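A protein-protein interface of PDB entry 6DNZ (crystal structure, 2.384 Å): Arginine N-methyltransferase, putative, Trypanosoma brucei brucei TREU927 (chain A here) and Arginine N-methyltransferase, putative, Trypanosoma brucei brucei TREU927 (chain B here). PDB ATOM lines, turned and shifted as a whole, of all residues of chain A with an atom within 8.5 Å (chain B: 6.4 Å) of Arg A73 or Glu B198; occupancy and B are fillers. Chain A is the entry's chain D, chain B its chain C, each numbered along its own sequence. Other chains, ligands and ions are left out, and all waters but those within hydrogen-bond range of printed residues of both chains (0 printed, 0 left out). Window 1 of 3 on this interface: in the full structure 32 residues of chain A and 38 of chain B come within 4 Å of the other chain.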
ATOM      1  N   ARG A  73     -17.832  22.674  -8.709  1.00  0.00           N
ATOM      2  CA  ARG A  73     -18.122  24.068  -9.020  1.00  0.00           C
ATOM      3  C   ARG A  73     -19.482  24.209  -9.704  1.00  0.00           C
ATOM      4  O   ARG A  73     -20.172  25.211  -9.522  1.00  0.00           O
ATOM      5  CB  ARG A  73     -17.016  24.660  -9.905  1.00  0.00           C
ATOM      6  CG  ARG A  73     -17.273  26.091 -10.383  1.00  0.00           C
ATOM      7  CD  ARG A  73     -17.404  27.074  -9.223  1.00  0.00           C
ATOM      8  NE  ARG A  73     -18.314  28.173  -9.537  1.00  0.00           N
ATOM      9  CZ  ARG A  73     -18.880  28.962  -8.628  1.00  0.00           C
ATOM     10  NH1 ARG A  73     -18.637  28.778  -7.335  1.00  0.00           N
ATOM     11  NH2 ARG A  73     -19.696  29.936  -9.011  1.00  0.00           N
ATOM     12  N   ILE A  74     -19.863  23.204 -10.495  1.00  0.00           N
ATOM     13  CA  ILE A  74     -21.153  23.246 -11.178  1.00  0.00           C
ATOM     14  C   ILE A  74     -22.291  23.148 -10.171  1.00  0.00           C
ATOM     15  O   ILE A  74     -23.304  23.847 -10.289  1.00  0.00           O
ATOM     16  CB  ILE A  74     -21.239  22.128 -12.233  1.00  0.00           C
ATOM     17  CG1 ILE A  74     -20.108  22.257 -13.259  1.00  0.00           C
ATOM     18  CG2 ILE A  74     -22.595  22.152 -12.926  1.00  0.00           C
ATOM     19  CD1 ILE A  74     -20.150  23.533 -14.079  1.00  0.00           C
ATOM     20  N   SER A  75     -22.147  22.279  -9.167  1.00  0.00           N
ATOM     21  CA  SER A  75     -23.199  22.114  -8.170  1.00  0.00           C
ATOM     22  C   SER A  75     -23.474  23.410  -7.420  1.00  0.00           C
ATOM     23  O   SER A  75     -24.611  23.653  -7.000  1.00  0.00           O
ATOM     24  CB  SER A  75     -22.816  21.010  -7.184  1.00  0.00           C
ATOM     25  OG  SER A  75     -21.575  21.295  -6.562  1.00  0.00           O
ATOM     26  N   GLY A  76     -22.454  24.250  -7.238  1.00  0.00           N
ATOM     27  CA  GLY A  76     -22.633  25.517  -6.550  1.00  0.00           C
ATOM     28  C   GLY A  76     -23.606  26.463  -7.224  1.00  0.00           C
ATOM     29  O   GLY A  76     -23.981  27.472  -6.615  1.00  0.00           O
ATOM     30  N   ASN A  77     -24.026  26.166  -8.452  1.00  0.00           N
ATOM     31  CA  ASN A  77     -24.943  27.020  -9.193  1.00  0.00           C
ATOM     32  C   ASN A  77     -26.385  26.534  -9.145  1.00  0.00           C
ATOM     33  O   ASN A  77     -27.267  27.201  -9.694  1.00  0.00           O
ATOM     34  CB  ASN A  77     -24.488  27.129 -10.651  1.00  0.00           C
ATOM     35  CG  ASN A  77     -23.071  27.647 -10.778  1.00  0.00           C
ATOM     36  OD1 ASN A  77     -22.128  26.874 -10.941  1.00  0.00           O
ATOM     37  ND2 ASN A  77     -22.913  28.964 -10.696  1.00  0.00           N
ATOM     38  N   LEU A  78     -26.647  25.390  -8.507  1.00  0.00           N
ATOM     39  CA  LEU A  78     -28.017  24.894  -8.405  1.00  0.00           C
ATOM     40  C   LEU A  78     -28.902  25.861  -7.631  1.00  0.00           C
ATOM     41  O   LEU A  78     -30.067  26.070  -7.988  1.00  0.00           O
ATOM     42  CB  LEU A  78     -28.026  23.523  -7.736  1.00  0.00           C
ATOM     43  CG  LEU A  78     -27.370  22.400  -8.533  1.00  0.00           C
ATOM     44  CD1 LEU A  78     -27.025  21.247  -7.619  1.00  0.00           C
ATOM     45  CD2 LEU A  78     -28.288  21.938  -9.650  1.00  0.00           C
ATOM     46  N   CYS A  80     -28.886  28.897  -7.751  1.00  0.00           N
ATOM     47  CA  CYS A  80     -29.279  30.000  -8.620  1.00  0.00           C
ATOM     48  C   CYS A  80     -30.503  29.639  -9.455  1.00  0.00           C
ATOM     49  O   CYS A  80     -31.468  30.407  -9.520  1.00  0.00           O
ATOM     50  CB  CYS A  80     -28.107  30.399  -9.520  1.00  0.00           C
ATOM     51  SG  CYS A  80     -28.373  31.934 -10.441  1.00  0.00           S
ATOM     52  N   GLY A 106     -20.527  39.923 -11.193  1.00  0.00           N
ATOM     53  CA  GLY A 106     -20.867  38.741 -10.419  1.00  0.00           C
ATOM     54  C   GLY A 106     -21.923  37.902 -11.102  1.00  0.00           C
ATOM     55  O   GLY A 106     -22.872  37.446 -10.452  1.00  0.00           O
ATOM     56  N   CYS A 107     -21.781  37.693 -12.413  1.00  0.00           N
ATOM     57  CA  CYS A 107     -22.800  36.993 -13.183  1.00  0.00           C
ATOM     58  C   CYS A 107     -22.898  35.518 -12.824  1.00  0.00           C
ATOM     59  O   CYS A 107     -23.920  34.890 -13.121  1.00  0.00           O
ATOM     60  CB  CYS A 107     -22.510  37.130 -14.678  1.00  0.00           C
ATOM     61  SG  CYS A 107     -20.998  36.293 -15.205  1.00  0.00           S
ATOM     62  N   GLY A 108     -21.869  34.954 -12.199  1.00  0.00           N
ATOM     63  CA  GLY A 108     -21.894  33.535 -11.894  1.00  0.00           C
ATOM     64  C   GLY A 108     -22.072  32.723 -13.160  1.00  0.00           C
ATOM     65  O   GLY A 108     -21.331  32.877 -14.136  1.00  0.00           O
ATOM     66  N   MET A 109     -23.072  31.850 -13.156  1.00  0.00           N
ATOM     67  CA  MET A 109     -23.365  31.019 -14.316  1.00  0.00           C
ATOM     68  C   MET A 109     -23.952  31.841 -15.461  1.00  0.00           C
ATOM     69  O   MET A 109     -24.045  31.366 -16.592  1.00  0.00           O
ATOM     70  CB  MET A 109     -24.330  29.901 -13.935  1.00  0.00           C
ATOM     71  CG  MET A 109     -25.610  30.390 -13.291  1.00  0.00           C
ATOM     72  SD  MET A 109     -26.868  28.934 -13.023  1.00  0.00           S
ATOM     73  CE  MET A 109     -27.227  28.493 -14.887  1.00  0.00           C
ATOM     74  N   GLY A 110     -24.357  33.071 -15.158  1.00  0.00           N
ATOM     75  CA  GLY A 110     -24.854  33.968 -16.183  1.00  0.00           C
ATOM     76  C   GLY A 110     -26.280  33.718 -16.613  1.00  0.00           C
ATOM     77  O   GLY A 110     -26.631  34.004 -17.762  1.00  0.00           O
ATOM     78  N   ASP A 128     -17.213  37.652 -14.089  1.00  0.00           N
ATOM     79  CA  ASP A 128     -17.081  36.931 -12.830  1.00  0.00           C
ATOM     80  C   ASP A 128     -15.681  36.343 -12.765  1.00  0.00           C
ATOM     81  O   ASP A 128     -15.062  36.078 -13.798  1.00  0.00           O
ATOM     82  CB  ASP A 128     -18.130  35.822 -12.690  1.00  0.00           C
ATOM     83  CG  ASP A 128     -18.313  35.373 -11.253  1.00  0.00           C
ATOM     84  OD1 ASP A 128     -19.202  35.919 -10.569  1.00  0.00           O
ATOM     85  OD2 ASP A 128     -17.561  34.482 -10.806  1.00  0.00           O
ATOM     86  N   ARG A 129     -15.191  36.141 -11.542  1.00  0.00           N
ATOM     87  CA  ARG A 129     -13.835  35.634 -11.361  1.00  0.00           C
ATOM     88  C   ARG A 129     -13.750  34.123 -11.542  1.00  0.00           C
ATOM     89  O   ARG A 129     -12.706  33.616 -11.967  1.00  0.00           O
ATOM     90  CB  ARG A 129     -13.311  36.018  -9.977  1.00  0.00           C
ATOM     91  CG  ARG A 129     -13.173  37.518  -9.754  1.00  0.00           C
ATOM     92  CD  ARG A 129     -12.695  37.828  -8.339  1.00  0.00           C
ATOM     93  NE  ARG A 129     -12.936  39.226  -7.972  1.00  0.00           N
ATOM     94  CZ  ARG A 129     -11.993  40.156  -7.824  1.00  0.00           C
ATOM     95  NH1 ARG A 129     -10.709  39.866  -7.996  1.00  0.00           N
ATOM     96  NH2 ARG A 129     -12.343  41.391  -7.488  1.00  0.00           N
ATOM     97  N   SER A 130     -14.817  33.392 -11.234  1.00  0.00           N
ATOM     98  CA  SER A 130     -14.773  31.939 -11.292  1.00  0.00           C
ATOM     99  C   SER A 130     -14.837  31.450 -12.734  1.00  0.00           C
ATOM    100  O   SER A 130     -15.409  32.102 -13.613  1.00  0.00           O
ATOM    101  CB  SER A 130     -15.920  31.329 -10.490  1.00  0.00           C
ATOM    102  OG  SER A 130     -17.156  31.518 -11.151  1.00  0.00           O
ATOM    103  N   ALA A 131     -14.250  30.273 -12.965  1.00  0.00           N
ATOM    104  CA  ALA A 131     -14.186  29.699 -14.303  1.00  0.00           C
ATOM    105  C   ALA A 131     -15.556  29.369 -14.878  1.00  0.00           C
ATOM    106  O   ALA A 131     -15.642  29.027 -16.062  1.00  0.00           O
ATOM    107  CB  ALA A 131     -13.329  28.431 -14.283  1.00  0.00           C
ATOM    108  N   ILE A 132     -16.624  29.459 -14.082  1.00  0.00           N
ATOM    109  CA  ILE A 132     -17.947  29.092 -14.577  1.00  0.00           C
ATOM    110  C   ILE A 132     -18.338  29.946 -15.776  1.00  0.00           C
ATOM    111  O   ILE A 132     -19.110  29.503 -16.635  1.00  0.00           O
ATOM    112  CB  ILE A 132     -18.984  29.204 -13.444  1.00  0.00           C
ATOM    113  CG1 ILE A 132     -20.284  28.489 -13.826  1.00  0.00           C
ATOM    114  CG2 ILE A 132     -19.272  30.659 -13.135  1.00  0.00           C
ATOM    115  CD1 ILE A 132     -20.163  26.979 -13.888  1.00  0.00           C
ATOM    116  N   VAL A 133     -17.820  31.175 -15.862  1.00  0.00           N
ATOM    117  CA  VAL A 133     -18.154  32.042 -16.992  1.00  0.00           C
ATOM    118  C   VAL A 133     -17.722  31.400 -18.303  1.00  0.00           C
ATOM    119  O   VAL A 133     -18.439  31.469 -19.309  1.00  0.00           O
ATOM    120  CB  VAL A 133     -17.522  33.435 -16.816  1.00  0.00           C
ATOM    121  CG1 VAL A 133     -18.108  34.121 -15.602  1.00  0.00           C
ATOM    122  CG2 VAL A 133     -16.005  33.337 -16.711  1.00  0.00           C
ATOM    123  N   ALA A 135     -17.672  28.251 -18.942  1.00  0.00           N
ATOM    124  CA  ALA A 135     -18.774  27.336 -19.212  1.00  0.00           C
ATOM    125  C   ALA A 135     -20.019  28.095 -19.653  1.00  0.00           C
ATOM    126  O   ALA A 135     -20.711  27.681 -20.589  1.00  0.00           O
ATOM    127  CB  ALA A 135     -19.068  26.496 -17.970  1.00  0.00           C
ATOM    128  N   ARG A 390     -14.892  37.213   4.121  1.00  0.00           N
ATOM    129  CA  ARG A 390     -15.429  36.631   2.899  1.00  0.00           C
ATOM    130  C   ARG A 390     -14.440  35.657   2.269  1.00  0.00           C
ATOM    131  O   ARG A 390     -14.807  34.529   1.928  1.00  0.00           O
ATOM    132  CB  ARG A 390     -15.793  37.745   1.911  1.00  0.00           C
ATOM    133  CG  ARG A 390     -16.344  37.259   0.575  1.00  0.00           C
ATOM    134  CD  ARG A 390     -17.689  36.569   0.729  1.00  0.00           C
ATOM    135  NE  ARG A 390     -18.159  36.024  -0.542  1.00  0.00           N
ATOM    136  CZ  ARG A 390     -17.818  34.829  -1.019  1.00  0.00           C
ATOM    137  NH1 ARG A 390     -17.002  34.038  -0.334  1.00  0.00           N
ATOM    138  NH2 ARG A 390     -18.297  34.426  -2.188  1.00  0.00           N
ATOM    139  N   TYR A 391     -13.186  36.077   2.120  1.00  0.00           N
ATOM    140  CA  TYR A 391     -12.146  35.241   1.526  1.00  0.00           C
ATOM    141  C   TYR A 391     -10.952  35.126   2.467  1.00  0.00           C
ATOM    142  O   TYR A 391     -10.765  35.965   3.350  1.00  0.00           O
ATOM    143  CB  TYR A 391     -11.696  35.817   0.181  1.00  0.00           C
ATOM    144  CG  TYR A 391     -12.777  35.837  -0.874  1.00  0.00           C
ATOM    145  CD1 TYR A 391     -13.528  34.703  -1.148  1.00  0.00           C
ATOM    146  CD2 TYR A 391     -13.050  36.992  -1.593  1.00  0.00           C
ATOM    147  CE1 TYR A 391     -14.517  34.714  -2.111  1.00  0.00           C
ATOM    148  CE2 TYR A 391     -14.039  37.014  -2.559  1.00  0.00           C
ATOM    149  CZ  TYR A 391     -14.769  35.873  -2.813  1.00  0.00           C
ATOM    150  OH  TYR A 391     -15.755  35.885  -3.772  1.00  0.00           O
ATOM    151  OXT TYR A 391     -10.144  34.200   2.366  1.00  0.00           O
ATOM    152  N   PHE B 177     -27.779  16.514 -12.391  1.00  0.00           N
ATOM    153  CA  PHE B 177     -27.332  16.375 -13.774  1.00  0.00           C
ATOM    154  C   PHE B 177     -28.430  16.726 -14.767  1.00  0.00           C
ATOM    155  O   PHE B 177     -28.262  17.661 -15.559  1.00  0.00           O
ATOM    156  CB  PHE B 177     -26.826  14.947 -14.015  1.00  0.00           C
ATOM    157  CG  PHE B 177     -25.578  14.607 -13.250  1.00  0.00           C
ATOM    158  CD1 PHE B 177     -25.651  14.144 -11.947  1.00  0.00           C
ATOM    159  CD2 PHE B 177     -24.331  14.753 -13.833  1.00  0.00           C
ATOM    160  CE1 PHE B 177     -24.504  13.832 -11.240  1.00  0.00           C
ATOM    161  CE2 PHE B 177     -23.181  14.442 -13.131  1.00  0.00           C
ATOM    162  CZ  PHE B 177     -23.268  13.981 -11.834  1.00  0.00           C
ATOM    163  N   LEU B 194     -20.383  18.764 -17.498  1.00  0.00           N
ATOM    164  CA  LEU B 194     -19.304  19.137 -16.592  1.00  0.00           C
ATOM    165  C   LEU B 194     -19.506  18.552 -15.200  1.00  0.00           C
ATOM    166  O   LEU B 194     -18.526  18.277 -14.498  1.00  0.00           O
ATOM    167  CB  LEU B 194     -19.191  20.658 -16.501  1.00  0.00           C
ATOM    168  CG  LEU B 194     -18.744  21.408 -17.755  1.00  0.00           C
ATOM    169  CD1 LEU B 194     -18.644  22.894 -17.451  1.00  0.00           C
ATOM    170  CD2 LEU B 194     -17.421  20.873 -18.278  1.00  0.00           C
ATOM    171  N   SER B 195     -20.758  18.363 -14.780  1.00  0.00           N
ATOM    172  CA  SER B 195     -21.016  17.832 -13.446  1.00  0.00           C
ATOM    173  C   SER B 195     -20.378  16.463 -13.254  1.00  0.00           C
ATOM    174  O   SER B 195     -19.978  16.117 -12.138  1.00  0.00           O
ATOM    175  CB  SER B 195     -22.522  17.751 -13.194  1.00  0.00           C
ATOM    176  OG  SER B 195     -23.118  19.036 -13.240  1.00  0.00           O
ATOM    177  N   PHE B 196     -20.272  15.673 -14.325  1.00  0.00           N
ATOM    178  CA  PHE B 196     -19.689  14.341 -14.215  1.00  0.00           C
ATOM    179  C   PHE B 196     -18.202  14.379 -13.887  1.00  0.00           C
ATOM    180  O   PHE B 196     -17.658  13.371 -13.426  1.00  0.00           O
ATOM    181  CB  PHE B 196     -19.908  13.562 -15.513  1.00  0.00           C
ATOM    182  CG  PHE B 196     -21.323  13.101 -15.711  1.00  0.00           C
ATOM    183  CD1 PHE B 196     -21.788  11.959 -15.080  1.00  0.00           C
ATOM    184  CD2 PHE B 196     -22.187  13.805 -16.531  1.00  0.00           C
ATOM    185  CE1 PHE B 196     -23.088  11.531 -15.260  1.00  0.00           C
ATOM    186  CE2 PHE B 196     -23.488  13.381 -16.716  1.00  0.00           C
ATOM    187  CZ  PHE B 196     -23.939  12.242 -16.079  1.00  0.00           C
ATOM    188  N   ILE B 197     -17.536  15.511 -14.111  1.00  0.00           N
ATOM    189  CA  ILE B 197     -16.106  15.596 -13.836  1.00  0.00           C
ATOM    190  C   ILE B 197     -15.843  15.703 -12.339  1.00  0.00           C
ATOM    191  O   ILE B 197     -14.790  15.268 -11.859  1.00  0.00           O
ATOM    192  CB  ILE B 197     -15.490  16.791 -14.586  1.00  0.00           C
ATOM    193  CG1 ILE B 197     -15.728  16.661 -16.093  1.00  0.00           C
ATOM    194  CG2 ILE B 197     -13.997  16.895 -14.289  1.00  0.00           C
ATOM    195  CD1 ILE B 197     -15.371  17.906 -16.875  1.00  0.00           C
ATOM    196  N   GLU B 198     -16.783  16.265 -11.583  1.00  0.00           N
ATOM    197  CA  GLU B 198     -16.540  16.624 -10.195  1.00  0.00           C
ATOM    198  C   GLU B 198     -17.055  15.528  -9.280  1.00  0.00           C
ATOM    199  O   GLU B 198     -18.271  15.289  -9.244  1.00  0.00           O
ATOM    200  CB  GLU B 198     -17.226  17.949  -9.869  1.00  0.00           C
ATOM    201  CG  GLU B 198     -16.933  19.056 -10.876  1.00  0.00           C
ATOM    202  CD  GLU B 198     -17.801  20.279 -10.666  1.00  0.00           C
ATOM    203  OE1 GLU B 198     -17.249  21.400 -10.616  1.00  0.00           O
ATOM    204  OE2 GLU B 198     -19.035  20.118 -10.544  1.00  0.00           O
ATOM    205  N   PRO B 199     -16.195  14.832  -8.536  1.00  0.00           N
ATOM    206  CA  PRO B 199     -16.696  13.885  -7.538  1.00  0.00           C
ATOM    207  C   PRO B 199     -17.536  14.591  -6.487  1.00  0.00           C
ATOM    208  O   PRO B 199     -17.418  15.797  -6.261  1.00  0.00           O
ATOM    209  CB  PRO B 199     -15.419  13.297  -6.927  1.00  0.00           C
ATOM    210  CG  PRO B 199     -14.395  13.470  -7.980  1.00  0.00           C
ATOM    211  CD  PRO B 199     -14.728  14.774  -8.643  1.00  0.00           C
ATOM    212  N   LEU B 200     -18.398  13.814  -5.843  1.00  0.00           N
ATOM    213  CA  LEU B 200     -19.279  14.307  -4.794  1.00  0.00           C
ATOM    214  C   LEU B 200     -18.852  13.688  -3.471  1.00  0.00           C
ATOM    215  O   LEU B 200     -18.819  12.461  -3.338  1.00  0.00           O
ATOM    216  CB  LEU B 200     -20.737  13.967  -5.106  1.00  0.00           C
ATOM    217  CG  LEU B 200     -21.773  14.262  -4.019  1.00  0.00           C
ATOM    218  CD1 LEU B 200     -22.199  15.720  -4.052  1.00  0.00           C
ATOM    219  CD2 LEU B 200     -22.977  13.337  -4.166  1.00  0.00           C
ATOM    220  N   VAL B 290     -18.158   9.955  -4.296  1.00  0.00           N
ATOM    221  CA  VAL B 290     -19.071   9.410  -5.293  1.00  0.00           C
ATOM    222  C   VAL B 290     -18.595   9.858  -6.666  1.00  0.00           C
ATOM    223  O   VAL B 290     -18.659  11.051  -6.995  1.00  0.00           O
ATOM    224  CB  VAL B 290     -20.517   9.852  -5.045  1.00  0.00           C
ATOM    225  CG1 VAL B 290     -21.451   9.168  -6.026  1.00  0.00           C
ATOM    226  CG2 VAL B 290     -20.921   9.553  -3.608  1.00  0.00           C
ATOM    227  N   LEU B 291     -18.130   8.907  -7.471  1.00  0.00           N
ATOM    228  CA  LEU B 291     -17.731   9.163  -8.850  1.00  0.00           C
ATOM    229  C   LEU B 291     -18.889   8.751  -9.751  1.00  0.00           C
ATOM    230  O   LEU B 291     -19.151   7.557  -9.929  1.00  0.00           O
ATOM    231  CB  LEU B 291     -16.458   8.398  -9.203  1.00  0.00           C
ATOM    232  CG  LEU B 291     -15.332   8.452  -8.170  1.00  0.00           C
ATOM    233  CD1 LEU B 291     -14.142   7.633  -8.635  1.00  0.00           C
ATOM    234  CD2 LEU B 291     -14.920   9.886  -7.902  1.00  0.00           C
ATOM    235  N   TYR B 292     -19.583   9.735 -10.313  1.00  0.00           N
ATOM    236  CA  TYR B 292     -20.740   9.459 -11.154  1.00  0.00           C
ATOM    237  C   TYR B 292     -20.287   9.030 -12.542  1.00  0.00           C
ATOM    238  O   TYR B 292     -19.513   9.732 -13.200  1.00  0.00           O
ATOM    239  CB  TYR B 292     -21.643  10.686 -11.236  1.00  0.00           C
ATOM    240  CG  TYR B 292     -22.420  10.927  -9.966  1.00  0.00           C
ATOM    241  CD1 TYR B 292     -21.915  11.741  -8.963  1.00  0.00           C
ATOM    242  CD2 TYR B 292     -23.654  10.326  -9.762  1.00  0.00           C
ATOM    243  CE1 TYR B 292     -22.620  11.956  -7.796  1.00  0.00           C
ATOM    244  CE2 TYR B 292     -24.366  10.534  -8.598  1.00  0.00           C
ATOM    245  CZ  TYR B 292     -23.845  11.350  -7.620  1.00  0.00           C
ATOM    246  OH  TYR B 292     -24.553  11.561  -6.459  1.00  0.00           O
ATOM    247  N   ASP B 341     -12.891  10.720 -16.996  1.00  0.00           N
ATOM    248  CA  ASP B 341     -11.953  11.440 -16.150  1.00  0.00           C
ATOM    249  C   ASP B 341     -12.713  12.216 -15.084  1.00  0.00           C
ATOM    250  O   ASP B 341     -13.740  12.840 -15.368  1.00  0.00           O
ATOM    251  CB  ASP B 341     -11.086  12.405 -16.970  1.00  0.00           C
ATOM    252  CG  ASP B 341     -10.070  11.685 -17.840  1.00  0.00           C
ATOM    253  OD1 ASP B 341      -9.636  10.576 -17.462  1.00  0.00           O
ATOM    254  OD2 ASP B 341      -9.702  12.234 -18.901  1.00  0.00           O
ATOM    255  N   PHE B 342     -12.206  12.157 -13.856  1.00  0.00           N
ATOM    256  CA  PHE B 342     -12.710  12.953 -12.750  1.00  0.00           C
ATOM    257  C   PHE B 342     -11.580  13.824 -12.221  1.00  0.00           C
ATOM    258  O   PHE B 342     -10.413  13.423 -12.228  1.00  0.00           O
ATOM    259  CB  PHE B 342     -13.255  12.076 -11.613  1.00  0.00           C
ATOM    260  CG  PHE B 342     -14.279  11.073 -12.055  1.00  0.00           C
ATOM    261  CD1 PHE B 342     -13.891   9.831 -12.530  1.00  0.00           C
ATOM    262  CD2 PHE B 342     -15.630  11.366 -11.986  1.00  0.00           C
ATOM    263  CE1 PHE B 342     -14.831   8.905 -12.935  1.00  0.00           C
ATOM    264  CE2 PHE B 342     -16.574  10.445 -12.388  1.00  0.00           C
ATOM    265  CZ  PHE B 342     -16.174   9.212 -12.863  1.00  0.00           C
ATOM    266  N   ARG B 343     -11.934  15.020 -11.762  1.00  0.00           N
ATOM    267  CA  ARG B 343     -10.969  15.944 -11.172  1.00  0.00           C
ATOM    268  C   ARG B 343     -11.478  16.349  -9.797  1.00  0.00           C
ATOM    269  O   ARG B 343     -12.501  17.033  -9.686  1.00  0.00           O
ATOM    270  CB  ARG B 343     -10.751  17.165 -12.064  1.00  0.00           C
ATOM    271  CG  ARG B 343      -9.501  17.076 -12.933  1.00  0.00           C
ATOM    272  CD  ARG B 343      -9.785  17.463 -14.376  1.00  0.00           C
ATOM    273  NE  ARG B 343      -8.577  17.424 -15.198  1.00  0.00           N
ATOM    274  CZ  ARG B 343      -8.012  16.309 -15.655  1.00  0.00           C
ATOM    275  NH1 ARG B 343      -8.534  15.123 -15.368  1.00  0.00           N
ATOM    276  NH2 ARG B 343      -6.914  16.382 -16.397  1.00  0.00           N
ATOM    277  N   LEU B 344     -10.773  15.915  -8.760  1.00  0.00           N
ATOM    278  CA  LEU B 344     -11.114  16.261  -7.382  1.00  0.00           C
ATOM    279  C   LEU B 344     -10.402  17.568  -7.058  1.00  0.00           C
ATOM    280  O   LEU B 344      -9.187  17.593  -6.848  1.00  0.00           O
ATOM    281  CB  LEU B 344     -10.715  15.133  -6.438  1.00  0.00           C
ATOM    282  CG  LEU B 344     -11.365  15.047  -5.057  1.00  0.00           C
ATOM    283  CD1 LEU B 344     -12.859  15.316  -5.112  1.00  0.00           C
ATOM    284  CD2 LEU B 344     -11.101  13.671  -4.472  1.00  0.00           C
ATOM    285  N   ARG B 345     -11.161  18.660  -7.037  1.00  0.00           N
ATOM    286  CA  ARG B 345     -10.595  19.995  -6.868  1.00  0.00           C
ATOM    287  C   ARG B 345     -11.359  20.791  -5.816  1.00  0.00           C
ATOM    288  O   ARG B 345     -10.820  21.716  -5.204  1.00  0.00           O
ATOM    289  CB  ARG B 345     -10.613  20.755  -8.197  1.00  0.00           C
ATOM    290  CG  ARG B 345      -9.956  20.018  -9.353  1.00  0.00           C
ATOM    291  CD  ARG B 345     -10.376  20.606 -10.693  1.00  0.00           C
ATOM    292  NE  ARG B 345     -11.815  20.481 -10.910  1.00  0.00           N
ATOM    293  CZ  ARG B 345     -12.433  20.762 -12.053  1.00  0.00           C
ATOM    294  NH1 ARG B 345     -11.741  21.185 -13.104  1.00  0.00           N
ATOM    295  NH2 ARG B 345     -13.749  20.614 -12.147  1.00  0.00           N
ATOM    296  OXT ARG B 345     -12.534  20.529  -5.556  1.00  0.00           O
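OE1 of Glu B198 lies within hydrogen-bond range of N of Ile A74 (3.2 Å). The side-chain carboxylate (OE2) of Glu B198 lies close to the backbone NH (N) of Arg A73 (3.4 Å).
Of chain B, only Glu B198 comes within 4 Å of Arg A73. Of the printed residues of chain B, Ala A135 touches Leu B194 (3.7 Å). Of the printed residues of chain A, Leu B194 touches Ile A74 and Ala A135. Of the printed residues of chain A, Ser B195 touches Ile A74 (3.2 Å). No residue of chain A comes within 4 Å of Pro B199. The nearest printed residue of chain B that does not touch Ala A135 is Ser B195 (8.9 Å).
Among the printed residues, pairs that only touch across the chains: Ile A74 with Ser B195 (3.2 Å), Ala A135 with Leu B194 (3.7 Å) and Ile A74 with Leu B194 (3.7 Å).
The backbone carbonyl oxygen (O) of Arg A73 sits close to the side-chain amide oxygen (OD1) of Asn A77, at 2.9 Å. OE1 of Glu B198 is in salt-bridge range of NH2 of Arg B345 (3.9 Å). O of Ile A74 lies close to OD1 of Asn A77, at 3.3 Å.
Of the 16 printed residues of chain B, 3 touch a printed residue of chain A. Hydrophobic or aromatic side chains of chain B within 4 Å of the printed part of chain A: Leu B194. Hydrophobic or aromatic side chains of chain A that line the printed part of chain B: Ile A74 and Ala A135. Among the printed residues, 5 pairs touch across the chains. Among the printed residues, no Asp or Glu carboxylate lies within 4 Å of a Lys or Arg side-chain nitrogen of the other chain.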
